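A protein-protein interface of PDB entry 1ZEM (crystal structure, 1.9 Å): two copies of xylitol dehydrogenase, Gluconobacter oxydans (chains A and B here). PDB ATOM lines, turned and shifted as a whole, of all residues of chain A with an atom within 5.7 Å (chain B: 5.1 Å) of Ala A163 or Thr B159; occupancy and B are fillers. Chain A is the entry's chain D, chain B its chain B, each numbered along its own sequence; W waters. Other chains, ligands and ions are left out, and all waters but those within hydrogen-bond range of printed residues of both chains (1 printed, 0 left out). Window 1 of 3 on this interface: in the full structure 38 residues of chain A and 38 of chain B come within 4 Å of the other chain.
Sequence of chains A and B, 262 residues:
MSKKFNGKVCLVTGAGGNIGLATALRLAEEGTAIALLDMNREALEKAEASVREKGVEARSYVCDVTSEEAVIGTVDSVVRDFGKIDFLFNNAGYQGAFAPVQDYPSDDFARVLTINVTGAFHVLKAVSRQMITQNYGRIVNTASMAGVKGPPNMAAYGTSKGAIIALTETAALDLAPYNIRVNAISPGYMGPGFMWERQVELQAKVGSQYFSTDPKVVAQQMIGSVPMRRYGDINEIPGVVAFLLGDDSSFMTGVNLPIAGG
Hydrophobic or aromatic side chains of chain B that line the printed part of chain A: Leu B113, Ala B155 and Ala B163.
Of the 13 printed residues of chain A, 6 touch a printed residue of chain B.
Hydrophobic or aromatic side chains of chain A within 4 Å of the printed part of chain B: Val A117, Ala A163, Ala A166 and Leu A167.
Along chain A the printed residues that touch a printed residue of chain B span positions 117 to 167.
Among the printed residues, 9 pairs touch across the chains.
Among the printed residues, no Asp or Glu carboxylate lies within 4 Å of a Lys or Arg side-chain nitrogen of the other chain.
Thr A159 touches Ala B163, and with the chains exchanged Ala A163 touches Thr B159.
Gly A162 touches its own counterpart, Gly B162.
Ala B163 touches its own counterpart, Ala A163.
8 positions are printed for both chains.
Of the 9 pairs that touch across the chains among the printed residues, 4 have their exchanged pair printed and touching as well.
Val A117 touches Leu B113.
CB of Ala B163 touches OG1 of Thr A159, 2.9 Å away.
C of Gly B162 touches C of Gly A162, at 3.9 Å.
Ala A163 touches Thr B159 (CB to O, 3.2 Å).
N of Ala A163 touches N of Ala B163 (3.9 Å).
O of Gly B158 touches CB of Ala A166, at 3.3 Å.
Thr B159 touches Ala A166 (CA to CB, 3.9 Å).
Ala B155 touches Leu A167.
CB of Leu A167 touches CG2 of Thr B159 (3.2 Å).
Water W1 lies within hydrogen-bond range of the backbone carbonyl oxygen of Ala B155 (2.8 Å), the backbone NH of Thr B159 (3.2 Å) and the backbone carbonyl oxygen of Ala A166 (3.3 Å).
Of chain A, only Ala A163, Ala A166 and Leu A167 come within 4 Å of Thr B159.
Of the printed residues of chain A, Gly B162 touches Gly A162.
Printed residues of chain B within 4 Å of Leu A167: Ala B155 and Thr B159.
Of the printed residues of chain A, Ala B155 touches Leu A167 (3.8 Å).
The nearest printed residue of chain A that does not touch Ala B163 is Gly A162 (4.1 Å).
The side-chain hydroxyl (OG1) of Thr B159 is in hydrogen-bond range of the backbone carbonyl oxygen (O) of Ala B156 (2.5 Å).
The backbone carbonyl oxygen (O) of Ala B155 sits close to the side-chain hydroxyl (OG1) of Thr B159, 3.1 Å away.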
ATOM      1  N   LEU A 113      -7.110  -7.098   5.676  1.00  0.00           N
ATOM      2  CA  LEU A 113      -5.911  -7.241   4.834  1.00  0.00           C
ATOM      3  C   LEU A 113      -5.574  -8.713   4.572  1.00  0.00           C
ATOM      4  O   LEU A 113      -5.221  -9.113   3.464  1.00  0.00           O
ATOM      5  CB  LEU A 113      -4.695  -6.604   5.499  1.00  0.00           C
ATOM      6  CG  LEU A 113      -4.632  -5.071   5.522  1.00  0.00           C
ATOM      7  CD1 LEU A 113      -3.277  -4.667   6.091  1.00  0.00           C
ATOM      8  CD2 LEU A 113      -4.753  -4.513   4.147  1.00  0.00           C
ATOM      9  N   VAL A 117      -6.141  -9.279   0.771  1.00  0.00           N
ATOM     10  CA  VAL A 117      -4.858  -9.125   0.115  1.00  0.00           C
ATOM     11  C   VAL A 117      -4.024 -10.392   0.164  1.00  0.00           C
ATOM     12  O   VAL A 117      -3.744 -10.968  -0.895  1.00  0.00           O
ATOM     13  CB  VAL A 117      -4.028  -7.945   0.692  1.00  0.00           C
ATOM     14  CG1 VAL A 117      -2.876  -7.587  -0.264  1.00  0.00           C
ATOM     15  CG2 VAL A 117      -4.945  -6.728   0.855  1.00  0.00           C
ATOM     16  N   GLY A 158     -10.661  -0.148   2.123  1.00  0.00           N
ATOM     17  CA  GLY A 158     -10.091   0.728   1.122  1.00  0.00           C
ATOM     18  C   GLY A 158      -8.629   0.414   0.900  1.00  0.00           C
ATOM     19  O   GLY A 158      -8.160   0.290  -0.226  1.00  0.00           O
ATOM     20  N   THR A 159      -7.893   0.283   1.984  1.00  0.00           N
ATOM     21  CA  THR A 159      -6.488  -0.021   1.832  1.00  0.00           C
ATOM     22  C   THR A 159      -6.323  -1.401   1.159  1.00  0.00           C
ATOM     23  O   THR A 159      -5.434  -1.577   0.316  1.00  0.00           O
ATOM     24  CB  THR A 159      -5.794   0.033   3.188  1.00  0.00           C
ATOM     25  OG1 THR A 159      -4.682  -0.852   3.213  1.00  0.00           O
ATOM     26  CG2 THR A 159      -6.705  -0.359   4.256  1.00  0.00           C
ATOM     27  N   SER A 160      -7.168  -2.371   1.515  1.00  0.00           N
ATOM     28  CA  SER A 160      -7.032  -3.707   0.906  1.00  0.00           C
ATOM     29  C   SER A 160      -7.264  -3.662  -0.605  1.00  0.00           C
ATOM     30  O   SER A 160      -6.555  -4.324  -1.389  1.00  0.00           O
ATOM     31  CB  SER A 160      -7.990  -4.716   1.608  1.00  0.00           C
ATOM     32  OG  SER A 160      -9.336  -4.666   1.156  1.00  0.00           O
ATOM     33  N   LYS A 161      -8.221  -2.851  -1.025  1.00  0.00           N
ATOM     34  CA  LYS A 161      -8.546  -2.814  -2.433  1.00  0.00           C
ATOM     35  C   LYS A 161      -7.532  -1.972  -3.204  1.00  0.00           C
ATOM     36  O   LYS A 161      -7.265  -2.224  -4.388  1.00  0.00           O
ATOM     37  CB  LYS A 161      -9.991  -2.342  -2.592  1.00  0.00           C
ATOM     38  CG  LYS A 161     -11.039  -3.347  -1.955  1.00  0.00           C
ATOM     39  CD  LYS A 161     -10.911  -4.811  -2.534  1.00  0.00           C
ATOM     40  CE  LYS A 161     -12.013  -5.784  -2.025  1.00  0.00           C
ATOM     41  NZ  LYS A 161     -11.976  -7.045  -2.834  1.00  0.00           N
ATOM     42  N   GLY A 162      -6.960  -0.958  -2.553  1.00  0.00           N
ATOM     43  CA  GLY A 162      -5.922  -0.181  -3.235  1.00  0.00           C
ATOM     44  C   GLY A 162      -4.685  -1.093  -3.432  1.00  0.00           C
ATOM     45  O   GLY A 162      -3.930  -0.979  -4.412  1.00  0.00           O
ATOM     46  N   ALA A 163      -4.477  -1.981  -2.478  1.00  0.00           N
ATOM     47  CA  ALA A 163      -3.379  -2.936  -2.510  1.00  0.00           C
ATOM     48  C   ALA A 163      -3.648  -3.885  -3.656  1.00  0.00           C
ATOM     49  O   ALA A 163      -2.732  -4.257  -4.416  1.00  0.00           O
ATOM     50  CB  ALA A 163      -3.349  -3.723  -1.195  1.00  0.00           C
ATOM     51  N   ILE A 164      -4.904  -4.297  -3.802  1.00  0.00           N
ATOM     52  CA  ILE A 164      -5.243  -5.210  -4.899  1.00  0.00           C
ATOM     53  C   ILE A 164      -4.953  -4.596  -6.292  1.00  0.00           C
ATOM     54  O   ILE A 164      -4.495  -5.309  -7.228  1.00  0.00           O
ATOM     55  CB  ILE A 164      -6.751  -5.638  -4.852  1.00  0.00           C
ATOM     56  CG1 ILE A 164      -6.959  -6.712  -3.776  1.00  0.00           C
ATOM     57  CG2 ILE A 164      -7.177  -6.200  -6.216  1.00  0.00           C
ATOM     58  CD1 ILE A 164      -6.136  -7.993  -4.066  1.00  0.00           C
ATOM     59  N   ILE A 165      -5.231  -3.305  -6.443  1.00  0.00           N
ATOM     60  CA  ILE A 165      -4.985  -2.601  -7.722  1.00  0.00           C
ATOM     61  C   ILE A 165      -3.460  -2.603  -8.064  1.00  0.00           C
ATOM     62  O   ILE A 165      -3.072  -2.844  -9.214  1.00  0.00           O
ATOM     63  CB  ILE A 165      -5.615  -1.155  -7.664  1.00  0.00           C
ATOM     64  CG1 ILE A 165      -7.145  -1.261  -7.658  1.00  0.00           C
ATOM     65  CG2 ILE A 165      -5.191  -0.278  -8.893  1.00  0.00           C
ATOM     66  CD1 ILE A 165      -7.856   0.113  -7.328  1.00  0.00           C
ATOM     67  N   ALA A 166      -2.610  -2.351  -7.073  1.00  0.00           N
ATOM     68  CA  ALA A 166      -1.171  -2.383  -7.307  1.00  0.00           C
ATOM     69  C   ALA A 166      -0.712  -3.820  -7.579  1.00  0.00           C
ATOM     70  O   ALA A 166       0.124  -4.048  -8.474  1.00  0.00           O
ATOM     71  CB  ALA A 166      -0.408  -1.831  -6.126  1.00  0.00           C
ATOM     72  N   LEU A 167      -1.285  -4.780  -6.862  1.00  0.00           N
ATOM     73  CA  LEU A 167      -0.899  -6.199  -6.997  1.00  0.00           C
ATOM     74  C   LEU A 167      -1.219  -6.601  -8.421  1.00  0.00           C
ATOM     75  O   LEU A 167      -0.413  -7.245  -9.072  1.00  0.00           O
ATOM     76  CB  LEU A 167      -1.679  -7.123  -6.042  1.00  0.00           C
ATOM     77  CG  LEU A 167      -1.315  -8.641  -6.079  1.00  0.00           C
ATOM     78  CD1 LEU A 167       0.251  -8.853  -5.969  1.00  0.00           C
ATOM     79  CD2 LEU A 167      -2.053  -9.388  -4.930  1.00  0.00           C
ATOM     80  N   THR A 168      -2.392  -6.181  -8.890  1.00  0.00           N
ATOM     81  CA  THR A 168      -2.795  -6.471 -10.252  1.00  0.00           C
ATOM     82  C   THR A 168      -1.773  -5.964 -11.267  1.00  0.00           C
ATOM     83  O   THR A 168      -1.452  -6.687 -12.220  1.00  0.00           O
ATOM     84  CB  THR A 168      -4.173  -5.860 -10.578  1.00  0.00           C
ATOM     85  OG1 THR A 168      -5.155  -6.438  -9.713  1.00  0.00           O
ATOM     86  CG2 THR A 168      -4.578  -6.186 -12.001  1.00  0.00           C
ATOM     87  N   PHE B 109       5.479 -11.890   2.183  1.00  0.00           N
ATOM     88  CA  PHE B 109       4.382 -11.091   1.688  1.00  0.00           C
ATOM     89  C   PHE B 109       3.556 -10.579   2.843  1.00  0.00           C
ATOM     90  O   PHE B 109       3.187  -9.414   2.879  1.00  0.00           O
ATOM     91  CB  PHE B 109       3.493 -11.923   0.752  1.00  0.00           C
ATOM     92  CG  PHE B 109       2.442 -11.112   0.060  1.00  0.00           C
ATOM     93  CD1 PHE B 109       2.641 -10.674  -1.243  1.00  0.00           C
ATOM     94  CD2 PHE B 109       1.232 -10.809   0.713  1.00  0.00           C
ATOM     95  CE1 PHE B 109       1.644  -9.956  -1.908  1.00  0.00           C
ATOM     96  CE2 PHE B 109       0.231 -10.086   0.076  1.00  0.00           C
ATOM     97  CZ  PHE B 109       0.424  -9.666  -1.226  1.00  0.00           C
ATOM     98  N   LEU B 113       3.172  -6.528   4.386  1.00  0.00           N
ATOM     99  CA  LEU B 113       1.893  -5.896   4.660  1.00  0.00           C
ATOM    100  C   LEU B 113       1.738  -5.523   6.113  1.00  0.00           C
ATOM    101  O   LEU B 113       1.213  -4.473   6.388  1.00  0.00           O
ATOM    102  CB  LEU B 113       0.683  -6.762   4.282  1.00  0.00           C
ATOM    103  CG  LEU B 113       0.330  -7.069   2.826  1.00  0.00           C
ATOM    104  CD1 LEU B 113      -1.092  -7.667   2.767  1.00  0.00           C
ATOM    105  CD2 LEU B 113       0.348  -5.805   1.980  1.00  0.00           C
ATOM    106  N   MET B 154       7.907  -6.946  -7.233  1.00  0.00           N
ATOM    107  CA  MET B 154       7.718  -6.320  -5.933  1.00  0.00           C
ATOM    108  C   MET B 154       6.291  -6.425  -5.549  1.00  0.00           C
ATOM    109  O   MET B 154       5.727  -5.456  -5.086  1.00  0.00           O
ATOM    110  CB  MET B 154       8.109  -4.818  -5.958  1.00  0.00           C
ATOM    111  CG  MET B 154       9.542  -4.508  -6.321  1.00  0.00           C
ATOM    112  SD  MET B 154       9.919  -2.744  -6.270  1.00  0.00           S
ATOM    113  CE  MET B 154      10.338  -2.497  -4.449  1.00  0.00           C
ATOM    114  N   ALA B 155       5.711  -7.596  -5.734  1.00  0.00           N
ATOM    115  CA  ALA B 155       4.317  -7.829  -5.404  1.00  0.00           C
ATOM    116  C   ALA B 155       3.843  -7.263  -4.058  1.00  0.00           C
ATOM    117  O   ALA B 155       2.912  -6.446  -4.006  1.00  0.00           O
ATOM    118  CB  ALA B 155       4.035  -9.289  -5.440  1.00  0.00           C
ATOM    119  N   ALA B 156       4.478  -7.688  -2.967  1.00  0.00           N
ATOM    120  CA  ALA B 156       4.073  -7.245  -1.643  1.00  0.00           C
ATOM    121  C   ALA B 156       4.337  -5.746  -1.376  1.00  0.00           C
ATOM    122  O   ALA B 156       3.429  -5.051  -0.907  1.00  0.00           O
ATOM    123  CB  ALA B 156       4.746  -8.146  -0.524  1.00  0.00           C
ATOM    124  N   TYR B 157       5.533  -5.250  -1.695  1.00  0.00           N
ATOM    125  CA  TYR B 157       5.846  -3.837  -1.456  1.00  0.00           C
ATOM    126  C   TYR B 157       4.886  -2.881  -2.203  1.00  0.00           C
ATOM    127  O   TYR B 157       4.280  -1.957  -1.597  1.00  0.00           O
ATOM    128  CB  TYR B 157       7.294  -3.559  -1.855  1.00  0.00           C
ATOM    129  CG  TYR B 157       7.720  -2.153  -1.492  1.00  0.00           C
ATOM    130  CD1 TYR B 157       8.011  -1.821  -0.176  1.00  0.00           C
ATOM    131  CD2 TYR B 157       7.826  -1.163  -2.461  1.00  0.00           C
ATOM    132  CE1 TYR B 157       8.399  -0.539   0.172  1.00  0.00           C
ATOM    133  CE2 TYR B 157       8.226   0.132  -2.128  1.00  0.00           C
ATOM    134  CZ  TYR B 157       8.507   0.438  -0.820  1.00  0.00           C
ATOM    135  OH  TYR B 157       8.910   1.724  -0.458  1.00  0.00           O
ATOM    136  N   GLY B 158       4.697  -3.133  -3.501  1.00  0.00           N
ATOM    137  CA  GLY B 158       3.800  -2.292  -4.285  1.00  0.00           C
ATOM    138  C   GLY B 158       2.374  -2.327  -3.738  1.00  0.00           C
ATOM    139  O   GLY B 158       1.716  -1.288  -3.648  1.00  0.00           O
ATOM    140  N   THR B 159       1.891  -3.504  -3.365  1.00  0.00           N
ATOM    141  CA  THR B 159       0.545  -3.606  -2.792  1.00  0.00           C
ATOM    142  C   THR B 159       0.480  -2.855  -1.431  1.00  0.00           C
ATOM    143  O   THR B 159      -0.497  -2.199  -1.150  1.00  0.00           O
ATOM    144  CB  THR B 159       0.173  -5.036  -2.528  1.00  0.00           C
ATOM    145  OG1 THR B 159       1.137  -5.598  -1.645  1.00  0.00           O
ATOM    146  CG2 THR B 159       0.178  -5.823  -3.817  1.00  0.00           C
ATOM    147  N   SER B 160       1.510  -2.963  -0.608  1.00  0.00           N
ATOM    148  CA  SER B 160       1.531  -2.251   0.672  1.00  0.00           C
ATOM    149  C   SER B 160       1.471  -0.717   0.458  1.00  0.00           C
ATOM    150  O   SER B 160       0.821  -0.006   1.219  1.00  0.00           O
ATOM    151  CB  SER B 160       2.783  -2.617   1.500  1.00  0.00           C
ATOM    152  OG  SER B 160       4.021  -1.983   1.082  1.00  0.00           O
ATOM    153  N   LYS B 161       2.129  -0.200  -0.564  1.00  0.00           N
ATOM    154  CA  LYS B 161       2.105   1.260  -0.764  1.00  0.00           C
ATOM    155  C   LYS B 161       0.853   1.733  -1.500  1.00  0.00           C
ATOM    156  O   LYS B 161       0.447   2.887  -1.366  1.00  0.00           O
ATOM    157  CB  LYS B 161       3.386   1.703  -1.447  1.00  0.00           C
ATOM    158  CG  LYS B 161       4.622   1.297  -0.603  1.00  0.00           C
ATOM    159  CD  LYS B 161       4.590   1.855   0.858  1.00  0.00           C
ATOM    160  CE  LYS B 161       5.998   2.006   1.407  1.00  0.00           C
ATOM    161  NZ  LYS B 161       6.020   2.794   2.708  1.00  0.00           N
ATOM    162  N   GLY B 162       0.237   0.814  -2.242  1.00  0.00           N
ATOM    163  CA  GLY B 162      -1.020   1.102  -2.924  1.00  0.00           C
ATOM    164  C   GLY B 162      -2.045   1.169  -1.775  1.00  0.00           C
ATOM    165  O   GLY B 162      -2.945   2.018  -1.761  1.00  0.00           O
ATOM    166  N   ALA B 163      -1.860   0.339  -0.751  1.00  0.00           N
ATOM    167  CA  ALA B 163      -2.745   0.376   0.385  1.00  0.00           C
ATOM    168  C   ALA B 163      -2.555   1.736   1.144  1.00  0.00           C
ATOM    169  O   ALA B 163      -3.509   2.394   1.584  1.00  0.00           O
ATOM    170  CB  ALA B 163      -2.429  -0.809   1.322  1.00  0.00           C
ATOM    171  N   ILE B 164      -1.311   2.163   1.285  1.00  0.00           N
ATOM    172  CA  ILE B 164      -1.053   3.415   2.005  1.00  0.00           C
ATOM    173  C   ILE B 164      -1.701   4.609   1.302  1.00  0.00           C
ATOM    174  O   ILE B 164      -2.238   5.546   1.956  1.00  0.00           O
ATOM    175  CB  ILE B 164       0.465   3.630   2.156  1.00  0.00           C
ATOM    176  CG1 ILE B 164       0.984   2.647   3.189  1.00  0.00           C
ATOM    177  CG2 ILE B 164       0.778   5.089   2.592  1.00  0.00           C
ATOM    178  CD1 ILE B 164       0.272   2.764   4.584  1.00  0.00           C
HETATM  179  O   HOH W   1       2.383  -4.798  -6.233  1.00  0.00           O
